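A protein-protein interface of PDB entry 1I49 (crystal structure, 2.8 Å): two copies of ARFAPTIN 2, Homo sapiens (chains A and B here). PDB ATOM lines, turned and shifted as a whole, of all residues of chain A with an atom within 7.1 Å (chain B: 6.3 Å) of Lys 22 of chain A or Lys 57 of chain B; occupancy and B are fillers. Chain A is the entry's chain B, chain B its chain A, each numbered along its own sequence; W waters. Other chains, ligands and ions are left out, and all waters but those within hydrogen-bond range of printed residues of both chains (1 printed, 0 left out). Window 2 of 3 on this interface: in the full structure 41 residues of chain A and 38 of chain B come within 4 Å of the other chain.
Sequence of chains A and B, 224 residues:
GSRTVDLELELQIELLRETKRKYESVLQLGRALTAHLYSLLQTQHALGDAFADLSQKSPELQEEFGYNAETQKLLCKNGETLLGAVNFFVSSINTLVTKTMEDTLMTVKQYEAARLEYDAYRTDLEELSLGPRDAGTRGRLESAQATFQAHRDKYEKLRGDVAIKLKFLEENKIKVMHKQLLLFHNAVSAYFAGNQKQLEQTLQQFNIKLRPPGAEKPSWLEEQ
The side-chain amino group (NZ) of Lys 22 of chain A lies within salt-bridge range of the side-chain carboxylate (OD2) of Asp 53 of chain B (3.6 Å).
OD1 of Asp 53 of chain B lies within salt-bridge range of NZ of Lys 57 of chain B, at 2.4 Å.
Among the printed residues, merely in contact across the chains: Lys 22 of chain A with Leu 54 of chain B (3.9 Å) and Lys 22 of chain A with Lys 57 of chain B (3.6 Å).
Glu 18 of chain A touches none of the printed residues of chain B. Lys 22 of chain A touches three residues of chain B. Leu 29 of chain A touches none of the printed residues of chain B. Printed residues of chain A within 4 Å of Asp 53 of chain B: Lys 22 (3.0 Å). Of the printed residues of chain A, Leu 54 of chain B touches Lys 22 (3.9 Å). Of the printed residues of chain A, Lys 57 of chain B touches Lys 22. The nearest residue of chain B that does not touch Lys 22 of chain A is Ala 50 of chain B (6.0 Å). The nearest residue of chain A that does not touch Lys 57 of chain B is Glu 18 of chain A (5.0 Å).
Of the 10 printed residues of chain B, 3 touch a printed residue of chain A. Hydrophobic or aromatic side chains of chain B that line the printed part of chain A: Leu 54. Printed residues of chain A that touch a printed residue of chain B: Lys 22. Among the printed residues, 3 pairs touch across the chains. Among the printed residues, Asp or Glu carboxylates within 4 Å of a Lys or Arg side-chain nitrogen of the other chain: Lys 22 of chain A with Asp 53 of chain B.
No position is printed for both chains.
Water W1 lies within hydrogen-bond range of the side-chain hydroxyl (OH) of Tyr 23 of chain A and the side-chain hydroxyl (OG) of Ser 58 of chain B.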
ATOM      1  N   LEU A  15      16.957  -8.111   7.184  1.00  0.00           N
ATOM      2  CA  LEU A  15      17.079  -8.452   8.588  1.00  0.00           C
ATOM      3  C   LEU A  15      18.423  -8.017   9.148  1.00  0.00           C
ATOM      4  O   LEU A  15      18.502  -7.488  10.257  1.00  0.00           O
ATOM      5  CB  LEU A  15      16.955  -9.957   8.777  1.00  0.00           C
ATOM      6  CG  LEU A  15      15.638 -10.498   9.297  1.00  0.00           C
ATOM      7  CD1 LEU A  15      14.595 -10.514   8.196  1.00  0.00           C
ATOM      8  CD2 LEU A  15      15.891 -11.884   9.826  1.00  0.00           C
ATOM      9  N   LEU A  16      19.484  -8.275   8.381  1.00  0.00           N
ATOM     10  CA  LEU A  16      20.826  -7.917   8.802  1.00  0.00           C
ATOM     11  C   LEU A  16      20.883  -6.408   8.962  1.00  0.00           C
ATOM     12  O   LEU A  16      21.408  -5.890   9.962  1.00  0.00           O
ATOM     13  CB  LEU A  16      21.864  -8.372   7.775  1.00  0.00           C
ATOM     14  CG  LEU A  16      23.282  -7.814   7.999  1.00  0.00           C
ATOM     15  CD1 LEU A  16      23.831  -8.299   9.334  1.00  0.00           C
ATOM     16  CD2 LEU A  16      24.190  -8.229   6.872  1.00  0.00           C
ATOM     17  N   ARG A  17      20.335  -5.697   7.981  1.00  0.00           N
ATOM     18  CA  ARG A  17      20.340  -4.248   8.042  1.00  0.00           C
ATOM     19  C   ARG A  17      19.576  -3.691   9.250  1.00  0.00           C
ATOM     20  O   ARG A  17      20.068  -2.789   9.935  1.00  0.00           O
ATOM     21  CB  ARG A  17      19.817  -3.682   6.733  1.00  0.00           C
ATOM     22  CG  ARG A  17      20.883  -3.682   5.664  1.00  0.00           C
ATOM     23  CD  ARG A  17      20.387  -3.129   4.361  1.00  0.00           C
ATOM     24  NE  ARG A  17      21.493  -2.861   3.449  1.00  0.00           N
ATOM     25  CZ  ARG A  17      21.466  -3.135   2.149  1.00  0.00           C
ATOM     26  NH1 ARG A  17      20.389  -3.680   1.613  1.00  0.00           N
ATOM     27  NH2 ARG A  17      22.518  -2.892   1.388  1.00  0.00           N
ATOM     28  N   GLU A  18      18.391  -4.226   9.528  1.00  0.00           N
ATOM     29  CA  GLU A  18      17.625  -3.758  10.673  1.00  0.00           C
ATOM     30  C   GLU A  18      18.353  -4.115  11.960  1.00  0.00           C
ATOM     31  O   GLU A  18      18.413  -3.314  12.899  1.00  0.00           O
ATOM     32  CB  GLU A  18      16.228  -4.377  10.692  1.00  0.00           C
ATOM     33  CG  GLU A  18      15.217  -3.669   9.817  1.00  0.00           C
ATOM     34  CD  GLU A  18      13.844  -4.285   9.930  1.00  0.00           C
ATOM     35  OE1 GLU A  18      13.397  -4.501  11.078  1.00  0.00           O
ATOM     36  OE2 GLU A  18      13.216  -4.549   8.881  1.00  0.00           O
ATOM     37  N   THR A  19      18.901  -5.322  12.010  1.00  0.00           N
ATOM     38  CA  THR A  19      19.625  -5.750  13.191  1.00  0.00           C
ATOM     39  C   THR A  19      20.796  -4.817  13.460  1.00  0.00           C
ATOM     40  O   THR A  19      20.939  -4.294  14.565  1.00  0.00           O
ATOM     41  CB  THR A  19      20.168  -7.164  13.023  1.00  0.00           C
ATOM     42  OG1 THR A  19      19.074  -8.083  13.007  1.00  0.00           O
ATOM     43  CG2 THR A  19      21.129  -7.518  14.171  1.00  0.00           C
ATOM     44  N   LYS A  20      21.629  -4.606  12.446  1.00  0.00           N
ATOM     45  CA  LYS A  20      22.782  -3.743  12.613  1.00  0.00           C
ATOM     46  C   LYS A  20      22.363  -2.358  13.113  1.00  0.00           C
ATOM     47  O   LYS A  20      22.973  -1.814  14.037  1.00  0.00           O
ATOM     48  CB  LYS A  20      23.562  -3.632  11.307  1.00  0.00           C
ATOM     49  CG  LYS A  20      24.822  -2.817  11.447  1.00  0.00           C
ATOM     50  CD  LYS A  20      25.699  -2.884  10.228  1.00  0.00           C
ATOM     51  CE  LYS A  20      26.655  -1.707  10.221  1.00  0.00           C
ATOM     52  NZ  LYS A  20      25.891  -0.415  10.142  1.00  0.00           N
ATOM     53  N   ARG A  21      21.324  -1.788  12.508  1.00  0.00           N
ATOM     54  CA  ARG A  21      20.830  -0.486  12.936  1.00  0.00           C
ATOM     55  C   ARG A  21      20.401  -0.533  14.402  1.00  0.00           C
ATOM     56  O   ARG A  21      20.777   0.341  15.180  1.00  0.00           O
ATOM     57  CB  ARG A  21      19.642  -0.044  12.075  1.00  0.00           C
ATOM     58  CG  ARG A  21      20.034   0.508  10.719  1.00  0.00           C
ATOM     59  CD  ARG A  21      18.866   1.225  10.042  1.00  0.00           C
ATOM     60  NE  ARG A  21      18.631   0.691   8.702  1.00  0.00           N
ATOM     61  CZ  ARG A  21      17.620  -0.112   8.390  1.00  0.00           C
ATOM     62  NH1 ARG A  21      16.753  -0.450   9.325  1.00  0.00           N
ATOM     63  NH2 ARG A  21      17.488  -0.588   7.157  1.00  0.00           N
ATOM     64  N   LYS A  22      19.619  -1.541  14.791  1.00  0.00           N
ATOM     65  CA  LYS A  22      19.181  -1.626  16.186  1.00  0.00           C
ATOM     66  C   LYS A  22      20.401  -1.763  17.105  1.00  0.00           C
ATOM     67  O   LYS A  22      20.475  -1.128  18.160  1.00  0.00           O
ATOM     68  CB  LYS A  22      18.246  -2.833  16.429  1.00  0.00           C
ATOM     69  CG  LYS A  22      16.992  -2.954  15.541  1.00  0.00           C
ATOM     70  CD  LYS A  22      16.124  -1.711  15.541  1.00  0.00           C
ATOM     71  CE  LYS A  22      14.649  -2.050  15.745  1.00  0.00           C
ATOM     72  NZ  LYS A  22      14.062  -2.880  14.677  1.00  0.00           N
ATOM     73  N   TYR A  23      21.356  -2.601  16.701  1.00  0.00           N
ATOM     74  CA  TYR A  23      22.555  -2.822  17.505  1.00  0.00           C
ATOM     75  C   TYR A  23      23.402  -1.558  17.653  1.00  0.00           C
ATOM     76  O   TYR A  23      24.118  -1.399  18.636  1.00  0.00           O
ATOM     77  CB  TYR A  23      23.400  -3.953  16.916  1.00  0.00           C
ATOM     78  CG  TYR A  23      22.930  -5.353  17.273  1.00  0.00           C
ATOM     79  CD1 TYR A  23      23.855  -6.380  17.509  1.00  0.00           C
ATOM     80  CD2 TYR A  23      21.573  -5.664  17.348  1.00  0.00           C
ATOM     81  CE1 TYR A  23      23.444  -7.675  17.809  1.00  0.00           C
ATOM     82  CE2 TYR A  23      21.149  -6.964  17.642  1.00  0.00           C
ATOM     83  CZ  TYR A  23      22.092  -7.960  17.871  1.00  0.00           C
ATOM     84  OH  TYR A  23      21.679  -9.239  18.167  1.00  0.00           O
ATOM     85  N   GLU A  24      23.325  -0.653  16.682  1.00  0.00           N
ATOM     86  CA  GLU A  24      24.087   0.584  16.778  1.00  0.00           C
ATOM     87  C   GLU A  24      23.423   1.461  17.834  1.00  0.00           C
ATOM     88  O   GLU A  24      24.096   2.206  18.547  1.00  0.00           O
ATOM     89  CB  GLU A  24      24.155   1.285  15.420  1.00  0.00           C
ATOM     90  CG  GLU A  24      24.887   0.447  14.384  1.00  0.00           C
ATOM     91  CD  GLU A  24      25.018   1.102  13.015  1.00  0.00           C
ATOM     92  OE1 GLU A  24      23.996   1.530  12.436  1.00  0.00           O
ATOM     93  OE2 GLU A  24      26.158   1.173  12.507  1.00  0.00           O
ATOM     94  N   SER A  25      22.104   1.356  17.954  1.00  0.00           N
ATOM     95  CA  SER A  25      21.407   2.128  18.968  1.00  0.00           C
ATOM     96  C   SER A  25      21.818   1.594  20.322  1.00  0.00           C
ATOM     97  O   SER A  25      22.162   2.361  21.224  1.00  0.00           O
ATOM     98  CB  SER A  25      19.898   2.010  18.821  1.00  0.00           C
ATOM     99  OG  SER A  25      19.383   3.185  18.230  1.00  0.00           O
ATOM    100  N   VAL A  26      21.792   0.277  20.472  1.00  0.00           N
ATOM    101  CA  VAL A  26      22.172  -0.320  21.735  1.00  0.00           C
ATOM    102  C   VAL A  26      23.559   0.153  22.081  1.00  0.00           C
ATOM    103  O   VAL A  26      23.843   0.475  23.228  1.00  0.00           O
ATOM    104  CB  VAL A  26      22.158  -1.839  21.650  1.00  0.00           C
ATOM    105  CG1 VAL A  26      22.783  -2.449  22.911  1.00  0.00           C
ATOM    106  CG2 VAL A  26      20.717  -2.313  21.455  1.00  0.00           C
ATOM    107  N   LEU A  27      24.412   0.230  21.068  1.00  0.00           N
ATOM    108  CA  LEU A  27      25.791   0.665  21.243  1.00  0.00           C
ATOM    109  C   LEU A  27      25.897   2.124  21.720  1.00  0.00           C
ATOM    110  O   LEU A  27      26.690   2.444  22.607  1.00  0.00           O
ATOM    111  CB  LEU A  27      26.520   0.480  19.924  1.00  0.00           C
ATOM    112  CG  LEU A  27      28.002   0.142  19.917  1.00  0.00           C
ATOM    113  CD1 LEU A  27      28.344  -0.844  21.032  1.00  0.00           C
ATOM    114  CD2 LEU A  27      28.321  -0.439  18.528  1.00  0.00           C
ATOM    115  N   GLN A  28      25.108   3.007  21.120  1.00  0.00           N
ATOM    116  CA  GLN A  28      25.111   4.409  21.505  1.00  0.00           C
ATOM    117  C   GLN A  28      24.651   4.515  22.958  1.00  0.00           C
ATOM    118  O   GLN A  28      25.306   5.132  23.798  1.00  0.00           O
ATOM    119  CB  GLN A  28      24.155   5.200  20.616  1.00  0.00           C
ATOM    120  CG  GLN A  28      24.669   5.529  19.237  1.00  0.00           C
ATOM    121  CD  GLN A  28      25.864   6.467  19.276  1.00  0.00           C
ATOM    122  OE1 GLN A  28      26.966   6.084  19.686  1.00  0.00           O
ATOM    123  NE2 GLN A  28      25.649   7.711  18.855  1.00  0.00           N
ATOM    124  N   LEU A  29      23.509   3.913  23.253  1.00  0.00           N
ATOM    125  CA  LEU A  29      22.998   3.946  24.606  1.00  0.00           C
ATOM    126  C   LEU A  29      24.079   3.432  25.554  1.00  0.00           C
ATOM    127  O   LEU A  29      24.321   4.012  26.609  1.00  0.00           O
ATOM    128  CB  LEU A  29      21.728   3.086  24.708  1.00  0.00           C
ATOM    129  CG  LEU A  29      20.557   3.538  23.806  1.00  0.00           C
ATOM    130  CD1 LEU A  29      19.363   2.628  23.997  1.00  0.00           C
ATOM    131  CD2 LEU A  29      20.156   4.964  24.123  1.00  0.00           C
ATOM    132  N   VAL A  97      29.445  -5.372  15.654  1.00  0.00           N
ATOM    133  CA  VAL A  97      28.736  -4.427  14.799  1.00  0.00           C
ATOM    134  C   VAL A  97      29.648  -3.746  13.786  1.00  0.00           C
ATOM    135  O   VAL A  97      29.463  -3.856  12.572  1.00  0.00           O
ATOM    136  CB  VAL A  97      28.049  -3.327  15.656  1.00  0.00           C
ATOM    137  CG1 VAL A  97      27.354  -2.326  14.769  1.00  0.00           C
ATOM    138  CG2 VAL A  97      27.050  -3.956  16.619  1.00  0.00           C
ATOM    139  N   ALA B  50      14.862  -0.559  24.129  1.00  0.00           N
ATOM    140  CA  ALA B  50      15.644  -1.170  23.055  1.00  0.00           C
ATOM    141  C   ALA B  50      15.788  -2.682  23.284  1.00  0.00           C
ATOM    142  O   ALA B  50      15.497  -3.485  22.388  1.00  0.00           O
ATOM    143  CB  ALA B  50      17.015  -0.515  22.967  1.00  0.00           C
ATOM    144  N   ALA B  52      13.931  -4.386  24.815  1.00  0.00           N
ATOM    145  CA  ALA B  52      12.581  -4.912  24.699  1.00  0.00           C
ATOM    146  C   ALA B  52      12.354  -5.223  23.239  1.00  0.00           C
ATOM    147  O   ALA B  52      12.283  -6.379  22.847  1.00  0.00           O
ATOM    148  CB  ALA B  52      11.559  -3.884  25.183  1.00  0.00           C
ATOM    149  N   ASP B  53      12.254  -4.164  22.443  1.00  0.00           N
ATOM    150  CA  ASP B  53      12.045  -4.258  21.009  1.00  0.00           C
ATOM    151  C   ASP B  53      12.859  -5.386  20.379  1.00  0.00           C
ATOM    152  O   ASP B  53      12.366  -6.062  19.483  1.00  0.00           O
ATOM    153  CB  ASP B  53      12.408  -2.932  20.354  1.00  0.00           C
ATOM    154  CG  ASP B  53      11.910  -2.829  18.930  1.00  0.00           C
ATOM    155  OD1 ASP B  53      10.684  -2.965  18.732  1.00  0.00           O
ATOM    156  OD2 ASP B  53      12.732  -2.608  18.015  1.00  0.00           O
ATOM    157  N   LEU B  54      14.092  -5.600  20.841  1.00  0.00           N
ATOM    158  CA  LEU B  54      14.911  -6.672  20.280  1.00  0.00           C
ATOM    159  C   LEU B  54      14.414  -8.056  20.691  1.00  0.00           C
ATOM    160  O   LEU B  54      14.404  -8.985  19.881  1.00  0.00           O
ATOM    161  CB  LEU B  54      16.386  -6.531  20.674  1.00  0.00           C
ATOM    162  CG  LEU B  54      17.368  -5.862  19.696  1.00  0.00           C
ATOM    163  CD1 LEU B  54      16.895  -6.081  18.274  1.00  0.00           C
ATOM    164  CD2 LEU B  54      17.461  -4.377  19.963  1.00  0.00           C
ATOM    165  N   SER B  55      14.013  -8.199  21.947  1.00  0.00           N
ATOM    166  CA  SER B  55      13.498  -9.475  22.438  1.00  0.00           C
ATOM    167  C   SER B  55      12.277  -9.911  21.611  1.00  0.00           C
ATOM    168  O   SER B  55      12.172 -11.056  21.169  1.00  0.00           O
ATOM    169  CB  SER B  55      13.099  -9.332  23.907  1.00  0.00           C
ATOM    170  OG  SER B  55      12.468 -10.505  24.375  1.00  0.00           O
ATOM    171  N   GLN B  56      11.365  -8.975  21.399  1.00  0.00           N
ATOM    172  CA  GLN B  56      10.157  -9.229  20.638  1.00  0.00           C
ATOM    173  C   GLN B  56      10.459  -9.553  19.177  1.00  0.00           C
ATOM    174  O   GLN B  56       9.739 -10.322  18.535  1.00  0.00           O
ATOM    175  CB  GLN B  56       9.257  -8.003  20.718  1.00  0.00           C
ATOM    176  CG  GLN B  56       7.883  -8.150  20.102  1.00  0.00           C
ATOM    177  CD  GLN B  56       6.925  -7.103  20.642  1.00  0.00           C
ATOM    178  OE1 GLN B  56       7.171  -5.901  20.529  1.00  0.00           O
ATOM    179  NE2 GLN B  56       5.833  -7.556  21.248  1.00  0.00           N
ATOM    180  N   LYS B  57      11.527  -8.970  18.652  1.00  0.00           N
ATOM    181  CA  LYS B  57      11.889  -9.186  17.265  1.00  0.00           C
ATOM    182  C   LYS B  57      12.988 -10.217  17.050  1.00  0.00           C
ATOM    183  O   LYS B  57      13.310 -10.549  15.914  1.00  0.00           O
ATOM    184  CB  LYS B  57      12.337  -7.871  16.649  1.00  0.00           C
ATOM    185  CG  LYS B  57      11.284  -6.787  16.565  1.00  0.00           C
ATOM    186  CD  LYS B  57      11.922  -5.557  15.934  1.00  0.00           C
ATOM    187  CE  LYS B  57      10.912  -4.530  15.424  1.00  0.00           C
ATOM    188  NZ  LYS B  57      10.185  -3.837  16.512  1.00  0.00           N
ATOM    189  N   SER B  58      13.554 -10.742  18.130  1.00  0.00           N
ATOM    190  CA  SER B  58      14.643 -11.698  17.995  1.00  0.00           C
ATOM    191  C   SER B  58      14.464 -13.022  18.729  1.00  0.00           C
ATOM    192  O   SER B  58      15.123 -13.278  19.739  1.00  0.00           O
ATOM    193  CB  SER B  58      15.945 -11.027  18.436  1.00  0.00           C
ATOM    194  OG  SER B  58      16.997 -11.965  18.549  1.00  0.00           O
ATOM    195  N   PRO B  59      13.599 -13.905  18.196  1.00  0.00           N
ATOM    196  CA  PRO B  59      13.304 -15.225  18.770  1.00  0.00           C
ATOM    197  C   PRO B  59      14.543 -16.018  19.146  1.00  0.00           C
ATOM    198  O   PRO B  59      14.547 -16.738  20.129  1.00  0.00           O
ATOM    199  CB  PRO B  59      12.514 -15.911  17.667  1.00  0.00           C
ATOM    200  CG  PRO B  59      11.776 -14.781  17.032  1.00  0.00           C
ATOM    201  CD  PRO B  59      12.847 -13.705  16.943  1.00  0.00           C
ATOM    202  N   GLU B  60      15.603 -15.893  18.365  1.00  0.00           N
ATOM    203  CA  GLU B  60      16.817 -16.633  18.670  1.00  0.00           C
ATOM    204  C   GLU B  60      17.469 -16.145  19.953  1.00  0.00           C
ATOM    205  O   GLU B  60      18.306 -16.846  20.537  1.00  0.00           O
ATOM    206  CB  GLU B  60      17.831 -16.514  17.524  1.00  0.00           C
ATOM    207  CG  GLU B  60      18.330 -15.103  17.212  1.00  0.00           C
ATOM    208  CD  GLU B  60      17.303 -14.258  16.458  1.00  0.00           C
ATOM    209  OE1 GLU B  60      17.684 -13.187  15.935  1.00  0.00           O
ATOM    210  OE2 GLU B  60      16.115 -14.658  16.384  1.00  0.00           O
HETATM  211  O   HOH W   1      19.024  -9.620  17.663  1.00  0.00           O
